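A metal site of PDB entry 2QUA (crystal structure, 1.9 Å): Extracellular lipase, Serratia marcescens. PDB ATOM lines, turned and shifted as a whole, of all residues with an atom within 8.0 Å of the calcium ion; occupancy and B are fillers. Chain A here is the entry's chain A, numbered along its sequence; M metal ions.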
ATOM      1  N   THR A 372     -13.683 -19.734 -24.358  1.00  0.00           N
ATOM      2  CA  THR A 372     -13.720 -18.766 -23.293  1.00  0.00           C
ATOM      3  C   THR A 372     -12.753 -17.633 -23.640  1.00  0.00           C
ATOM      4  O   THR A 372     -11.599 -17.859 -24.042  1.00  0.00           O
ATOM      5  CB  THR A 372     -13.360 -19.403 -21.955  1.00  0.00           C
ATOM      6  OG1 THR A 372     -14.228 -20.513 -21.735  1.00  0.00           O
ATOM      7  CG2 THR A 372     -13.493 -18.381 -20.776  1.00  0.00           C
ATOM      8  N   LYS A 384      -5.777 -16.916 -16.027  1.00  0.00           N
ATOM      9  CA  LYS A 384      -5.701 -18.372 -16.174  1.00  0.00           C
ATOM     10  C   LYS A 384      -6.834 -18.968 -17.011  1.00  0.00           C
ATOM     11  O   LYS A 384      -8.023 -18.861 -16.655  1.00  0.00           O
ATOM     12  CB  LYS A 384      -5.678 -19.089 -14.824  1.00  0.00           C
ATOM     13  CG  LYS A 384      -5.599 -20.606 -14.994  1.00  0.00           C
ATOM     14  CD  LYS A 384      -5.351 -21.354 -13.691  1.00  0.00           C
ATOM     15  CE  LYS A 384      -5.506 -22.889 -13.886  1.00  0.00           C
ATOM     16  NZ  LYS A 384      -6.893 -23.236 -14.405  1.00  0.00           N
ATOM     17  N   GLY A 385      -6.448 -19.610 -18.098  1.00  0.00           N
ATOM     18  CA  GLY A 385      -7.396 -20.337 -18.942  1.00  0.00           C
ATOM     19  C   GLY A 385      -7.668 -21.749 -18.467  1.00  0.00           C
ATOM     20  O   GLY A 385      -6.859 -22.360 -17.766  1.00  0.00           O
ATOM     21  N   GLY A 386      -8.824 -22.293 -18.864  1.00  0.00           N
ATOM     22  CA  GLY A 386      -9.213 -23.623 -18.444  1.00  0.00           C
ATOM     23  C   GLY A 386      -8.743 -24.734 -19.354  1.00  0.00           C
ATOM     24  O   GLY A 386      -7.868 -24.535 -20.188  1.00  0.00           O
ATOM     25  N   LYS A 387      -9.324 -25.919 -19.159  1.00  0.00           N
ATOM     26  CA  LYS A 387      -8.943 -27.118 -19.905  1.00  0.00           C
ATOM     27  C   LYS A 387      -9.497 -27.116 -21.307  1.00  0.00           C
ATOM     28  O   LYS A 387      -9.098 -27.945 -22.096  1.00  0.00           O
ATOM     29  CB  LYS A 387      -9.439 -28.376 -19.183  1.00  0.00           C
ATOM     30  CG  LYS A 387      -8.672 -28.656 -17.890  1.00  0.00           C
ATOM     31  CD  LYS A 387      -8.965 -30.053 -17.382  1.00  0.00           C
ATOM     32  CE  LYS A 387      -8.320 -30.239 -16.019  1.00  0.00           C
ATOM     33  NZ  LYS A 387      -8.748 -29.135 -15.089  1.00  0.00           N
ATOM     34  N   GLY A 388     -10.431 -26.210 -21.598  1.00  0.00           N
ATOM     35  CA  GLY A 388     -11.016 -26.101 -22.916  1.00  0.00           C
ATOM     36  C   GLY A 388     -10.234 -25.082 -23.739  1.00  0.00           C
ATOM     37  O   GLY A 388      -9.058 -24.810 -23.462  1.00  0.00           O
ATOM     38  N   ASN A 389     -10.901 -24.537 -24.739  1.00  0.00           N
ATOM     39  CA  ASN A 389     -10.245 -23.603 -25.642  1.00  0.00           C
ATOM     40  C   ASN A 389     -10.440 -22.185 -25.115  1.00  0.00           C
ATOM     41  O   ASN A 389     -11.579 -21.769 -24.826  1.00  0.00           O
ATOM     42  CB  ASN A 389     -10.801 -23.764 -27.059  1.00  0.00           C
ATOM     43  CG  ASN A 389     -10.734 -25.204 -27.519  1.00  0.00           C
ATOM     44  OD1 ASN A 389      -9.812 -25.949 -27.133  1.00  0.00           O
ATOM     45  ND2 ASN A 389     -11.708 -25.618 -28.327  1.00  0.00           N
ATOM     46  N   ASP A 390      -9.320 -21.466 -24.988  1.00  0.00           N
ATOM     47  CA  ASP A 390      -9.286 -20.145 -24.368  1.00  0.00           C
ATOM     48  C   ASP A 390      -8.618 -19.117 -25.271  1.00  0.00           C
ATOM     49  O   ASP A 390      -7.705 -19.436 -26.031  1.00  0.00           O
ATOM     50  CB  ASP A 390      -8.509 -20.226 -23.053  1.00  0.00           C
ATOM     51  CG  ASP A 390      -9.261 -20.968 -21.977  1.00  0.00           C
ATOM     52  OD1 ASP A 390     -10.052 -20.321 -21.259  1.00  0.00           O
ATOM     53  OD2 ASP A 390      -9.073 -22.202 -21.841  1.00  0.00           O
ATOM     54  N   TYR A 391      -9.116 -17.885 -25.194  1.00  0.00           N
ATOM     55  CA  TYR A 391      -8.531 -16.710 -25.851  1.00  0.00           C
ATOM     56  C   TYR A 391      -8.212 -15.710 -24.746  1.00  0.00           C
ATOM     57  O   TYR A 391      -9.134 -15.098 -24.169  1.00  0.00           O
ATOM     58  CB  TYR A 391      -9.529 -16.138 -26.867  1.00  0.00           C
ATOM     59  CG  TYR A 391      -9.833 -17.113 -27.956  1.00  0.00           C
ATOM     60  CD1 TYR A 391      -9.255 -16.989 -29.216  1.00  0.00           C
ATOM     61  CD2 TYR A 391     -10.692 -18.187 -27.739  1.00  0.00           C
ATOM     62  CE1 TYR A 391      -9.526 -17.893 -30.238  1.00  0.00           C
ATOM     63  CE2 TYR A 391     -10.964 -19.107 -28.754  1.00  0.00           C
ATOM     64  CZ  TYR A 391     -10.377 -18.951 -29.997  1.00  0.00           C
ATOM     65  OH  TYR A 391     -10.647 -19.844 -31.007  1.00  0.00           O
ATOM     66  N   LEU A 392      -6.920 -15.544 -24.440  1.00  0.00           N
ATOM     67  CA  LEU A 392      -6.497 -14.730 -23.304  1.00  0.00           C
ATOM     68  C   LEU A 392      -5.822 -13.466 -23.788  1.00  0.00           C
ATOM     69  O   LEU A 392      -4.867 -13.521 -24.573  1.00  0.00           O
ATOM     70  CB  LEU A 392      -5.510 -15.514 -22.445  1.00  0.00           C
ATOM     71  CG  LEU A 392      -6.003 -16.937 -22.106  1.00  0.00           C
ATOM     72  CD1 LEU A 392      -4.931 -17.691 -21.271  1.00  0.00           C
ATOM     73  CD2 LEU A 392      -7.373 -16.958 -21.410  1.00  0.00           C
ATOM     74  N   ARG A 402      -1.475 -18.496 -17.381  1.00  0.00           N
ATOM     75  CA  ARG A 402      -1.501 -19.921 -17.144  1.00  0.00           C
ATOM     76  C   ARG A 402      -2.632 -20.463 -18.030  1.00  0.00           C
ATOM     77  O   ARG A 402      -3.546 -19.720 -18.376  1.00  0.00           O
ATOM     78  CB  ARG A 402      -1.851 -20.181 -15.677  1.00  0.00           C
ATOM     79  CG  ARG A 402      -0.641 -20.022 -14.779  1.00  0.00           C
ATOM     80  CD  ARG A 402      -0.974 -20.243 -13.294  1.00  0.00           C
ATOM     81  NE  ARG A 402       0.246 -20.156 -12.534  1.00  0.00           N
ATOM     82  CZ  ARG A 402       0.335 -20.254 -11.216  1.00  0.00           C
ATOM     83  NH1 ARG A 402      -0.760 -20.454 -10.495  1.00  0.00           N
ATOM     84  NH2 ARG A 402       1.505 -20.152 -10.617  1.00  0.00           N
ATOM     85  N   ASP A 403      -2.584 -21.731 -18.413  1.00  0.00           N
ATOM     86  CA  ASP A 403      -3.716 -22.330 -19.098  1.00  0.00           C
ATOM     87  C   ASP A 403      -3.690 -23.839 -18.888  1.00  0.00           C
ATOM     88  O   ASP A 403      -2.617 -24.466 -18.987  1.00  0.00           O
ATOM     89  CB  ASP A 403      -3.752 -22.006 -20.604  1.00  0.00           C
ATOM     90  CG  ASP A 403      -4.982 -22.589 -21.275  1.00  0.00           C
ATOM     91  OD1 ASP A 403      -6.003 -21.872 -21.442  1.00  0.00           O
ATOM     92  OD2 ASP A 403      -4.995 -23.797 -21.614  1.00  0.00           O
ATOM     93  N   ALA A 404      -4.856 -24.411 -18.606  1.00  0.00           N
ATOM     94  CA  ALA A 404      -4.920 -25.774 -18.110  1.00  0.00           C
ATOM     95  C   ALA A 404      -5.022 -26.822 -19.213  1.00  0.00           C
ATOM     96  O   ALA A 404      -4.930 -28.008 -18.934  1.00  0.00           O
ATOM     97  CB  ALA A 404      -6.103 -25.922 -17.103  1.00  0.00           C
ATOM     98  N   GLY A 405      -5.207 -26.386 -20.460  1.00  0.00           N
ATOM     99  CA  GLY A 405      -5.205 -27.336 -21.573  1.00  0.00           C
ATOM    100  C   GLY A 405      -5.956 -26.884 -22.829  1.00  0.00           C
ATOM    101  O   GLY A 405      -6.324 -25.724 -22.951  1.00  0.00           O
ATOM    102  N   GLY A 406      -6.171 -27.814 -23.745  1.00  0.00           N
ATOM    103  CA  GLY A 406      -6.952 -27.539 -24.947  1.00  0.00           C
ATOM    104  C   GLY A 406      -6.196 -26.709 -25.963  1.00  0.00           C
ATOM    105  O   GLY A 406      -4.960 -26.760 -26.051  1.00  0.00           O
ATOM    106  N   TYR A 407      -6.920 -25.930 -26.760  1.00  0.00           N
ATOM    107  CA  TYR A 407      -6.333 -25.218 -27.894  1.00  0.00           C
ATOM    108  C   TYR A 407      -6.576 -23.728 -27.659  1.00  0.00           C
ATOM    109  O   TYR A 407      -7.722 -23.309 -27.482  1.00  0.00           O
ATOM    110  CB  TYR A 407      -6.954 -25.707 -29.218  1.00  0.00           C
ATOM    111  CG  TYR A 407      -6.632 -27.173 -29.479  1.00  0.00           C
ATOM    112  CD1 TYR A 407      -5.572 -27.519 -30.316  1.00  0.00           C
ATOM    113  CD2 TYR A 407      -7.373 -28.204 -28.884  1.00  0.00           C
ATOM    114  CE1 TYR A 407      -5.250 -28.852 -30.558  1.00  0.00           C
ATOM    115  CE2 TYR A 407      -7.066 -29.552 -29.119  1.00  0.00           C
ATOM    116  CZ  TYR A 407      -5.997 -29.861 -29.959  1.00  0.00           C
ATOM    117  OH  TYR A 407      -5.659 -31.149 -30.212  1.00  0.00           O
ATOM    118  N   ASN A 408      -5.496 -22.938 -27.650  1.00  0.00           N
ATOM    119  CA  ASN A 408      -5.595 -21.571 -27.113  1.00  0.00           C
ATOM    120  C   ASN A 408      -4.833 -20.522 -27.898  1.00  0.00           C
ATOM    121  O   ASN A 408      -3.805 -20.830 -28.533  1.00  0.00           O
ATOM    122  CB  ASN A 408      -5.059 -21.532 -25.661  1.00  0.00           C
ATOM    123  CG  ASN A 408      -5.537 -22.711 -24.841  1.00  0.00           C
ATOM    124  OD1 ASN A 408      -6.690 -22.761 -24.365  1.00  0.00           O
ATOM    125  ND2 ASN A 408      -4.649 -23.681 -24.646  1.00  0.00           N
ATOM    126  N   LEU A 409      -5.331 -19.284 -27.851  1.00  0.00           N
ATOM    127  CA  LEU A 409      -4.603 -18.106 -28.353  1.00  0.00           C
ATOM    128  C   LEU A 409      -4.371 -17.149 -27.227  1.00  0.00           C
ATOM    129  O   LEU A 409      -5.280 -16.896 -26.400  1.00  0.00           O
ATOM    130  CB  LEU A 409      -5.352 -17.354 -29.453  1.00  0.00           C
ATOM    131  CG  LEU A 409      -5.644 -18.064 -30.771  1.00  0.00           C
ATOM    132  CD1 LEU A 409      -6.352 -17.078 -31.627  1.00  0.00           C
ATOM    133  CD2 LEU A 409      -4.372 -18.576 -31.459  1.00  0.00           C
ATOM    134  N   ILE A 410      -3.174 -16.573 -27.192  1.00  0.00           N
ATOM    135  CA  ILE A 410      -2.825 -15.676 -26.120  1.00  0.00           C
ATOM    136  C   ILE A 410      -2.187 -14.441 -26.702  1.00  0.00           C
ATOM    137  O   ILE A 410      -1.220 -14.546 -27.457  1.00  0.00           O
ATOM    138  CB  ILE A 410      -1.874 -16.334 -25.101  1.00  0.00           C
ATOM    139  CG1 ILE A 410      -2.553 -17.560 -24.486  1.00  0.00           C
ATOM    140  CG2 ILE A 410      -1.418 -15.291 -24.059  1.00  0.00           C
ATOM    141  CD1 ILE A 410      -1.772 -18.233 -23.420  1.00  0.00           C
ATOM    142  N   ASP A 441       1.066 -29.382 -25.555  1.00  0.00           N
ATOM    143  CA  ASP A 441       1.111 -30.209 -24.372  1.00  0.00           C
ATOM    144  C   ASP A 441       1.098 -31.711 -24.693  1.00  0.00           C
ATOM    145  O   ASP A 441       1.027 -32.125 -25.855  1.00  0.00           O
ATOM    146  CB  ASP A 441       0.005 -29.818 -23.362  1.00  0.00           C
ATOM    147  CG  ASP A 441      -1.410 -30.145 -23.836  1.00  0.00           C
ATOM    148  OD1 ASP A 441      -1.599 -31.143 -24.571  1.00  0.00           O
ATOM    149  OD2 ASP A 441      -2.339 -29.388 -23.463  1.00  0.00           O
ATOM    150  N   ILE A 446      -2.660 -27.310 -28.399  1.00  0.00           N
ATOM    151  CA  ILE A 446      -1.715 -26.321 -28.880  1.00  0.00           C
ATOM    152  C   ILE A 446      -2.088 -24.902 -28.486  1.00  0.00           C
ATOM    153  O   ILE A 446      -3.236 -24.480 -28.666  1.00  0.00           O
ATOM    154  CB  ILE A 446      -1.568 -26.442 -30.418  1.00  0.00           C
ATOM    155  CG1 ILE A 446      -0.952 -27.801 -30.809  1.00  0.00           C
ATOM    156  CG2 ILE A 446      -0.790 -25.233 -30.975  1.00  0.00           C
ATOM    157  CD1 ILE A 446      -0.954 -28.059 -32.346  1.00  0.00           C
ATOM    158  N   THR A 447      -1.106 -24.170 -27.978  1.00  0.00           N
ATOM    159  CA  THR A 447      -1.253 -22.746 -27.665  1.00  0.00           C
ATOM    160  C   THR A 447      -0.366 -21.862 -28.556  1.00  0.00           C
ATOM    161  O   THR A 447       0.845 -22.120 -28.689  1.00  0.00           O
ATOM    162  CB  THR A 447      -0.854 -22.464 -26.202  1.00  0.00           C
ATOM    163  OG1 THR A 447      -1.665 -23.234 -25.316  1.00  0.00           O
ATOM    164  CG2 THR A 447      -1.004 -20.974 -25.884  1.00  0.00           C
HETATM  165 CA    CA M   1      -7.316 -23.681 -22.283  1.00  0.00          CA
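N of Asn 408 is in hydrogen-bond range of O of Ile 446 (2.9 Å). The backbone NH (N) of Asp 390 sits at hydrogen-bond distance from the backbone carbonyl oxygen (O) of Tyr 407 (3.5 Å). The backbone carbonyl oxygen of Gly 386 lies close to the backbone NH of Ala 404, at 3.4 Å. The backbone carbonyl oxygen (O) of Gly 406 sits at hydrogen-bond distance from the side-chain amide nitrogen (ND2) of Asn 408. O of Asp 390 is in hydrogen-bond range of N of Leu 409, at 3.0 Å. The side-chain amide nitrogen (ND2) of Asn 408 lies within hydrogen-bond range of the side-chain hydroxyl (OG1) of Thr 447 (3.1 Å).
The calcium ion is bound by O of Gly 386, at 2.3 Å. OD2 of Asp 390 binds the calcium ion (2.3 Å). OD1 of Asn 408 is bound to the calcium ion. O of Gly 405 binds the calcium ion, 2.4 Å away. The calcium ion is bound by the backbone carbonyl oxygen (O) of Gly 388 (2.4 Å). The side-chain carboxylate (OD1) of Asp 403 is bound to the calcium ion (2.4 Å). The side-chain carboxylate (OD2) of Asp 403 is bound to the calcium ion, at 2.4 Å. The calcium ion has seven donor atoms within binding distance.
Within 4 Å of the calcium ion: Gly 386, Gly 388, Asp 390, Asp 403, Gly 405 and Asn 408. Along chain A the residues within 4 Å of the calcium ion span positions 386 to 408.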
